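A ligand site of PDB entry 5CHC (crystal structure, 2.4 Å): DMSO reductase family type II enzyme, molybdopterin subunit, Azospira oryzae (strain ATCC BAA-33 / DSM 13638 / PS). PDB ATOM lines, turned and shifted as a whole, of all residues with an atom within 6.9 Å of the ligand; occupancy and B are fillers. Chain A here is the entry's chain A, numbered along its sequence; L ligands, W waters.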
ATOM      1  N   ALA A  31      14.277   6.894  -3.806  1.00  0.00           N
ATOM      2  CA  ALA A  31      13.501   7.940  -3.146  1.00  0.00           C
ATOM      3  C   ALA A  31      13.653   9.260  -3.899  1.00  0.00           C
ATOM      4  O   ALA A  31      14.567   9.447  -4.689  1.00  0.00           O
ATOM      5  CB  ALA A  31      13.930   8.094  -1.706  1.00  0.00           C
ATOM      6  N   HIS A  32      12.721  10.167  -3.674  1.00  0.00           N
ATOM      7  CA  HIS A  32      12.766  11.490  -4.271  1.00  0.00           C
ATOM      8  C   HIS A  32      13.168  12.491  -3.199  1.00  0.00           C
ATOM      9  O   HIS A  32      12.369  12.836  -2.308  1.00  0.00           O
ATOM     10  CB  HIS A  32      11.420  11.813  -4.918  1.00  0.00           C
ATOM     11  CG  HIS A  32      10.969  10.763  -5.877  1.00  0.00           C
ATOM     12  ND1 HIS A  32       9.781  10.062  -5.726  1.00  0.00           N
ATOM     13  CD2 HIS A  32      11.593  10.211  -6.941  1.00  0.00           C
ATOM     14  CE1 HIS A  32       9.674   9.157  -6.691  1.00  0.00           C
ATOM     15  NE2 HIS A  32      10.760   9.225  -7.443  1.00  0.00           N
ATOM     16  N   LEU A  33      14.414  12.953  -3.270  1.00  0.00           N
ATOM     17  CA  LEU A  33      14.979  13.815  -2.250  1.00  0.00           C
ATOM     18  C   LEU A  33      14.590  15.293  -2.448  1.00  0.00           C
ATOM     19  O   LEU A  33      15.449  16.143  -2.692  1.00  0.00           O
ATOM     20  CB  LEU A  33      16.507  13.663  -2.221  1.00  0.00           C
ATOM     21  CG  LEU A  33      17.011  12.221  -2.109  1.00  0.00           C
ATOM     22  CD1 LEU A  33      18.531  12.136  -1.958  1.00  0.00           C
ATOM     23  CD2 LEU A  33      16.326  11.494  -0.947  1.00  0.00           C
ATOM     24  N   VAL A  34      13.293  15.590  -2.318  1.00  0.00           N
ATOM     25  CA  VAL A  34      12.777  16.959  -2.442  1.00  0.00           C
ATOM     26  C   VAL A  34      11.864  17.320  -1.266  1.00  0.00           C
ATOM     27  O   VAL A  34      11.418  16.440  -0.514  1.00  0.00           O
ATOM     28  CB  VAL A  34      11.982  17.163  -3.749  1.00  0.00           C
ATOM     29  CG1 VAL A  34      12.900  17.163  -5.003  1.00  0.00           C
ATOM     30  CG2 VAL A  34      10.884  16.124  -3.865  1.00  0.00           C
ATOM     31  N   ASN A  35      11.595  18.608  -1.097  1.00  0.00           N
ATOM     32  CA  ASN A  35      10.893  19.072   0.095  1.00  0.00           C
ATOM     33  C   ASN A  35       9.365  18.954  -0.081  1.00  0.00           C
ATOM     34  O   ASN A  35       8.665  19.946  -0.162  1.00  0.00           O
ATOM     35  CB  ASN A  35      11.281  20.518   0.428  1.00  0.00           C
ATOM     36  CG  ASN A  35      10.773  20.964   1.803  1.00  0.00           C
ATOM     37  OD1 ASN A  35      10.531  20.136   2.685  1.00  0.00           O
ATOM     38  ND2 ASN A  35      10.589  22.270   1.984  1.00  0.00           N
ATOM     39  N   CYS A  36       8.860  17.731  -0.099  1.00  0.00           N
ATOM     40  CA  CYS A  36       7.449  17.487  -0.388  1.00  0.00           C
ATOM     41  C   CYS A  36       6.673  16.889   0.793  1.00  0.00           C
ATOM     42  O   CYS A  36       5.423  16.878   0.779  1.00  0.00           O
ATOM     43  CB  CYS A  36       7.335  16.537  -1.553  1.00  0.00           C
ATOM     44  SG  CYS A  36       8.182  15.002  -1.129  1.00  0.00           S
ATOM     45  N   THR A  37       7.401  16.375   1.780  1.00  0.00           N
ATOM     46  CA  THR A  37       6.856  15.616   2.945  1.00  0.00           C
ATOM     47  C   THR A  37       6.279  14.220   2.596  1.00  0.00           C
ATOM     48  O   THR A  37       5.666  13.585   3.440  1.00  0.00           O
ATOM     49  CB  THR A  37       5.749  16.399   3.712  1.00  0.00           C
ATOM     50  OG1 THR A  37       4.506  16.369   2.976  1.00  0.00           O
ATOM     51  CG2 THR A  37       6.170  17.841   3.952  1.00  0.00           C
ATOM     52  N   GLY A  38       6.504  13.733   1.386  1.00  0.00           N
ATOM     53  CA  GLY A  38       6.095  12.384   1.015  1.00  0.00           C
ATOM     54  C   GLY A  38       6.956  11.285   1.612  1.00  0.00           C
ATOM     55  O   GLY A  38       6.417  10.349   2.231  1.00  0.00           O
ATOM     56  N   ALA A  39       8.281  11.391   1.423  1.00  0.00           N
ATOM     57  CA  ALA A  39       9.233  10.356   1.803  1.00  0.00           C
ATOM     58  C   ALA A  39       8.669   8.990   1.462  1.00  0.00           C
ATOM     59  O   ALA A  39       8.647   8.065   2.285  1.00  0.00           O
ATOM     60  CB  ALA A  39       9.556  10.453   3.277  1.00  0.00           C
ATOM     61  N   CYS A  40       8.200   8.893   0.233  1.00  0.00           N
ATOM     62  CA  CYS A  40       7.477   7.729  -0.268  1.00  0.00           C
ATOM     63  C   CYS A  40       8.356   6.575  -0.740  1.00  0.00           C
ATOM     64  O   CYS A  40       9.159   6.747  -1.659  1.00  0.00           O
ATOM     65  CB  CYS A  40       6.571   8.170  -1.400  1.00  0.00           C
ATOM     66  SG  CYS A  40       5.334   9.373  -0.902  1.00  0.00           S
ATOM     67  N   PRO A  41       8.202   5.393  -0.121  1.00  0.00           N
ATOM     68  CA  PRO A  41       9.009   4.254  -0.584  1.00  0.00           C
ATOM     69  C   PRO A  41       8.734   3.899  -2.068  1.00  0.00           C
ATOM     70  O   PRO A  41       7.609   3.853  -2.544  1.00  0.00           O
ATOM     71  CB  PRO A  41       8.590   3.119   0.360  1.00  0.00           C
ATOM     72  CG  PRO A  41       8.128   3.811   1.612  1.00  0.00           C
ATOM     73  CD  PRO A  41       7.420   5.058   1.099  1.00  0.00           C
ATOM     74  N   HIS A  42       9.817   3.663  -2.805  1.00  0.00           N
ATOM     75  CA  HIS A  42       9.730   3.414  -4.223  1.00  0.00           C
ATOM     76  C   HIS A  42      10.693   2.327  -4.652  1.00  0.00           C
ATOM     77  O   HIS A  42      11.753   2.141  -4.035  1.00  0.00           O
ATOM     78  CB  HIS A  42      10.019   4.683  -5.035  1.00  0.00           C
ATOM     79  CG  HIS A  42       8.809   5.509  -5.327  1.00  0.00           C
ATOM     80  ND1 HIS A  42       8.294   6.419  -4.426  1.00  0.00           N
ATOM     81  CD2 HIS A  42       7.998   5.550  -6.420  1.00  0.00           C
ATOM     82  CE1 HIS A  42       7.215   6.985  -4.952  1.00  0.00           C
ATOM     83  NE2 HIS A  42       7.017   6.475  -6.157  1.00  0.00           N
ATOM     84  N   GLN A  56       5.822   3.020  -6.684  1.00  0.00           N
ATOM     85  CA  GLN A  56       5.661   2.850  -5.244  1.00  0.00           C
ATOM     86  C   GLN A  56       5.921   1.398  -4.829  1.00  0.00           C
ATOM     87  O   GLN A  56       5.424   0.488  -5.458  1.00  0.00           O
ATOM     88  CB  GLN A  56       4.252   3.262  -4.787  1.00  0.00           C
ATOM     89  CG  GLN A  56       3.866   4.711  -5.058  1.00  0.00           C
ATOM     90  CD  GLN A  56       3.046   4.862  -6.302  1.00  0.00           C
ATOM     91  OE1 GLN A  56       3.457   4.398  -7.368  1.00  0.00           O
ATOM     92  NE2 GLN A  56       1.880   5.505  -6.186  1.00  0.00           N
ATOM     93  N   ARG A  72       1.105   5.495  -1.198  1.00  0.00           N
ATOM     94  CA  ARG A  72       1.746   6.801  -1.284  1.00  0.00           C
ATOM     95  C   ARG A  72       2.129   7.087  -2.748  1.00  0.00           C
ATOM     96  O   ARG A  72       1.523   6.526  -3.673  1.00  0.00           O
ATOM     97  CB  ARG A  72       2.972   6.888  -0.373  1.00  0.00           C
ATOM     98  CG  ARG A  72       2.659   6.723   1.121  1.00  0.00           C
ATOM     99  CD  ARG A  72       3.852   7.121   2.024  1.00  0.00           C
ATOM    100  NE  ARG A  72       3.997   8.556   2.144  1.00  0.00           N
ATOM    101  CZ  ARG A  72       3.213   9.332   2.904  1.00  0.00           C
ATOM    102  NH1 ARG A  72       2.234   8.781   3.605  1.00  0.00           N
ATOM    103  NH2 ARG A  72       3.419  10.639   2.962  1.00  0.00           N
ATOM    104  N   GLY A  73       3.113   7.959  -2.950  1.00  0.00           N
ATOM    105  CA  GLY A  73       3.483   8.335  -4.297  1.00  0.00           C
ATOM    106  C   GLY A  73       2.736   9.580  -4.723  1.00  0.00           C
ATOM    107  O   GLY A  73       1.910  10.113  -3.949  1.00  0.00           O
ATOM    108  N   CYS A  74       3.012  10.041  -5.932  1.00  0.00           N
ATOM    109  CA  CYS A  74       2.309  11.172  -6.526  1.00  0.00           C
ATOM    110  C   CYS A  74       2.735  11.333  -7.973  1.00  0.00           C
ATOM    111  O   CYS A  74       3.585  10.580  -8.454  1.00  0.00           O
ATOM    112  CB  CYS A  74       2.581  12.479  -5.770  1.00  0.00           C
ATOM    113  SG  CYS A  74       4.066  13.320  -6.326  1.00  0.00           S
ATOM    114  N   ASN A  75       2.171  12.327  -8.634  1.00  0.00           N
ATOM    115  CA  ASN A  75       2.377  12.545 -10.063  1.00  0.00           C
ATOM    116  C   ASN A  75       3.812  12.966 -10.419  1.00  0.00           C
ATOM    117  O   ASN A  75       4.341  12.570 -11.456  1.00  0.00           O
ATOM    118  CB  ASN A  75       1.346  13.580 -10.583  1.00  0.00           C
ATOM    119  CG  ASN A  75       1.291  14.858  -9.724  1.00  0.00           C
ATOM    120  OD1 ASN A  75       1.460  14.821  -8.505  1.00  0.00           O
ATOM    121  ND2 ASN A  75       1.060  15.990 -10.375  1.00  0.00           N
ATOM    122  N   LYS A  76       4.470  13.739  -9.550  1.00  0.00           N
ATOM    123  CA  LYS A  76       5.869  14.060  -9.817  1.00  0.00           C
ATOM    124  C   LYS A  76       6.713  12.800  -9.662  1.00  0.00           C
ATOM    125  O   LYS A  76       7.612  12.531 -10.482  1.00  0.00           O
ATOM    126  CB  LYS A  76       6.395  15.154  -8.867  1.00  0.00           C
ATOM    127  CG  LYS A  76       5.801  16.516  -9.158  1.00  0.00           C
ATOM    128  CD  LYS A  76       4.374  16.648  -8.650  1.00  0.00           C
ATOM    129  CE  LYS A  76       4.373  16.763  -7.129  1.00  0.00           C
ATOM    130  NZ  LYS A  76       3.062  16.397  -6.544  1.00  0.00           N
ATOM    131  N   GLY A  77       6.421  12.050  -8.618  1.00  0.00           N
ATOM    132  CA  GLY A  77       7.259  10.929  -8.234  1.00  0.00           C
ATOM    133  C   GLY A  77       7.343   9.848  -9.284  1.00  0.00           C
ATOM    134  O   GLY A  77       8.429   9.353  -9.582  1.00  0.00           O
ATOM    135  N   GLU A  78       6.193   9.510  -9.895  1.00  0.00           N
ATOM    136  CA  GLU A  78       6.167   8.496 -10.927  1.00  0.00           C
ATOM    137  C   GLU A  78       6.780   8.964 -12.254  1.00  0.00           C
ATOM    138  O   GLU A  78       6.725   8.245 -13.262  1.00  0.00           O
ATOM    139  CB  GLU A  78       4.732   8.013 -11.152  1.00  0.00           C
ATOM    140  CG  GLU A  78       4.000   7.553  -9.887  1.00  0.00           C
ATOM    141  CD  GLU A  78       4.926   6.942  -8.823  1.00  0.00           C
ATOM    142  OE1 GLU A  78       5.692   6.001  -9.145  1.00  0.00           O
ATOM    143  OE2 GLU A  78       4.901   7.416  -7.664  1.00  0.00           O
ATOM    144  N   ILE A 209      -0.759  15.026  -1.045  1.00  0.00           N
ATOM    145  CA  ILE A 209      -1.269  13.991  -1.936  1.00  0.00           C
ATOM    146  C   ILE A 209      -1.117  12.529  -1.419  1.00  0.00           C
ATOM    147  O   ILE A 209      -2.096  11.781  -1.427  1.00  0.00           O
ATOM    148  CB  ILE A 209      -0.621  14.157  -3.336  1.00  0.00           C
ATOM    149  CG1 ILE A 209      -1.208  15.435  -3.985  1.00  0.00           C
ATOM    150  CG2 ILE A 209      -0.811  12.912  -4.229  1.00  0.00           C
ATOM    151  CD1 ILE A 209      -0.614  15.833  -5.340  1.00  0.00           C
ATOM    152  N   PRO A 210       0.075  12.125  -0.929  1.00  0.00           N
ATOM    153  CA  PRO A 210       0.135  10.713  -0.528  1.00  0.00           C
ATOM    154  C   PRO A 210      -0.664  10.376   0.743  1.00  0.00           C
ATOM    155  O   PRO A 210      -1.070   9.215   0.917  1.00  0.00           O
ATOM    156  CB  PRO A 210       1.646  10.474  -0.319  1.00  0.00           C
ATOM    157  CG  PRO A 210       2.248  11.831  -0.171  1.00  0.00           C
ATOM    158  CD  PRO A 210       1.405  12.761  -0.938  1.00  0.00           C
ATOM    159  N   GLN A 460       9.188  19.411   4.931  1.00  0.00           N
ATOM    160  CA  GLN A 460       9.894  18.254   5.467  1.00  0.00           C
ATOM    161  C   GLN A 460      10.924  18.663   6.494  1.00  0.00           C
ATOM    162  O   GLN A 460      12.120  18.407   6.353  1.00  0.00           O
ATOM    163  CB  GLN A 460      10.558  17.451   4.340  1.00  0.00           C
ATOM    164  CG  GLN A 460      10.308  15.964   4.433  1.00  0.00           C
ATOM    165  CD  GLN A 460      10.470  15.240   3.111  1.00  0.00           C
ATOM    166  OE1 GLN A 460       9.917  15.648   2.095  1.00  0.00           O
ATOM    167  NE2 GLN A 460      11.219  14.150   3.122  1.00  0.00           N
ATOM    168  N   ASN A 591      15.924   9.311   3.961  1.00  0.00           N
ATOM    169  CA  ASN A 591      14.829  10.174   3.531  1.00  0.00           C
ATOM    170  C   ASN A 591      13.686  10.056   4.540  1.00  0.00           C
ATOM    171  O   ASN A 591      13.056   9.007   4.625  1.00  0.00           O
ATOM    172  CB  ASN A 591      14.389   9.797   2.108  1.00  0.00           C
ATOM    173  CG  ASN A 591      13.257  10.689   1.540  1.00  0.00           C
ATOM    174  OD1 ASN A 591      12.177  10.204   1.206  1.00  0.00           O
ATOM    175  ND2 ASN A 591      13.526  11.981   1.406  1.00  0.00           N
ATOM    176  N   ASN A 600      12.766   6.042   5.141  1.00  0.00           N
ATOM    177  CA  ASN A 600      12.898   5.779   3.708  1.00  0.00           C
ATOM    178  C   ASN A 600      14.336   6.029   3.298  1.00  0.00           C
ATOM    179  O   ASN A 600      15.105   6.573   4.071  1.00  0.00           O
ATOM    180  CB  ASN A 600      11.938   6.666   2.898  1.00  0.00           C
ATOM    181  CG  ASN A 600      11.673   6.153   1.495  1.00  0.00           C
ATOM    182  OD1 ASN A 600      11.694   4.940   1.246  1.00  0.00           O
ATOM    183  ND2 ASN A 600      11.384   7.072   0.581  1.00  0.00           N
ATOM    184  N   VAL A 769       6.894  20.106  -7.031  1.00  0.00           N
ATOM    185  CA  VAL A 769       7.375  20.222  -5.661  1.00  0.00           C
ATOM    186  C   VAL A 769       8.251  21.466  -5.619  1.00  0.00           C
ATOM    187  O   VAL A 769       9.387  21.437  -6.099  1.00  0.00           O
ATOM    188  CB  VAL A 769       8.179  18.991  -5.230  1.00  0.00           C
ATOM    189  CG1 VAL A 769       8.779  19.203  -3.844  1.00  0.00           C
ATOM    190  CG2 VAL A 769       7.320  17.747  -5.285  1.00  0.00           C
ATOM    191  N   PHE A 773      10.287  20.097 -10.757  1.00  0.00           N
ATOM    192  CA  PHE A 773       9.172  19.622 -11.589  1.00  0.00           C
ATOM    193  C   PHE A 773       8.341  20.751 -12.193  1.00  0.00           C
ATOM    194  O   PHE A 773       7.442  20.463 -12.985  1.00  0.00           O
ATOM    195  CB  PHE A 773       8.244  18.648 -10.824  1.00  0.00           C
ATOM    196  CG  PHE A 773       8.906  17.350 -10.438  1.00  0.00           C
ATOM    197  CD1 PHE A 773       8.922  16.274 -11.316  1.00  0.00           C
ATOM    198  CD2 PHE A 773       9.543  17.208  -9.221  1.00  0.00           C
ATOM    199  CE1 PHE A 773       9.558  15.093 -10.987  1.00  0.00           C
ATOM    200  CE2 PHE A 773      10.163  16.017  -8.869  1.00  0.00           C
ATOM    201  CZ  PHE A 773      10.176  14.962  -9.767  1.00  0.00           C
HETATM  202 FE1  LIG L   1       5.720  12.635  -4.867  1.00  0.00          FE
HETATM  203 FE2  LIG L   1       7.451  13.495  -2.821  1.00  0.00          FE
HETATM  204 FE3  LIG L   1       8.281  11.346  -4.497  1.00  0.00          FE
HETATM  205 FE4  LIG L   1       6.168  10.895  -2.541  1.00  0.00          FE
HETATM  206  S1  LIG L   1       8.274  11.533  -2.332  1.00  0.00           S
HETATM  207  S2  LIG L   1       6.277  10.547  -4.666  1.00  0.00           S
HETATM  208  S3  LIG L   1       5.373  12.931  -2.741  1.00  0.00           S
HETATM  209  S4  LIG L   1       7.761  13.430  -4.914  1.00  0.00           S
HETATM  210  O   HOH W   1      10.600   9.614  -1.803  1.00  0.00           O
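CA of Gly 38 touches FE4 of the ligand (3.9 Å). His 42 touches the ligand (CE1 to S2, 3.7 Å). Gly 73 touches the ligand. Gly 77 touches the ligand (CA to S2, 3.7 Å). Nine residues have an atom within 4 Å of the ligand: His 32, Cys 36, Gly 38, Ala 39, Cys 40, His 42, Gly 73, Cys 74 and Gly 77.
N of Cys 74 lies close to S2 of the ligand, 3.5 Å away. The side-chain sulfur (SG) of Cys 74 binds an iron atom (FE1) of the ligand (2.3 Å). A ring nitrogen (ND1) of His 32 is bound to an iron atom (FE3) of the ligand (2.3 Å). An iron atom (FE2) of the ligand is bound by the side-chain sulfur (SG) of Cys 36 (2.4 Å). N of Cys 40 lies close to S1 of the ligand. SG of Cys 40 is bound to FE4 of the ligand (2.4 Å). A sulfur (S1) of the ligand lies close to the backbone NH (N) of Ala 39 (3.8 Å).
The side-chain sulfur (SG) of Cys 74 lies close to the backbone NH (N) of Gly 77 (3.5 Å). The side-chain sulfur (SG) of Cys 74 sits close to the side-chain amino group (NZ) of Lys 76 (3.2 Å). O of Val 34 lies close to SG of Cys 36 (3.6 Å). SG of Cys 40 lies close to N of Gly 73 (3.3 Å). The side-chain sulfur (SG) of Cys 40 sits close to the backbone carbonyl oxygen (O) of Gly 38 (3.5 Å). SG of Cys 40 lies close to NE of Arg 72 (3.4 Å). O of Ala 39 lies within hydrogen-bond range of ND2 of Asn 600 (3.4 Å). The guanidinium group of Arg 72 is in hydrogen-bond range of the backbone carbonyl oxygen of Gly 38.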
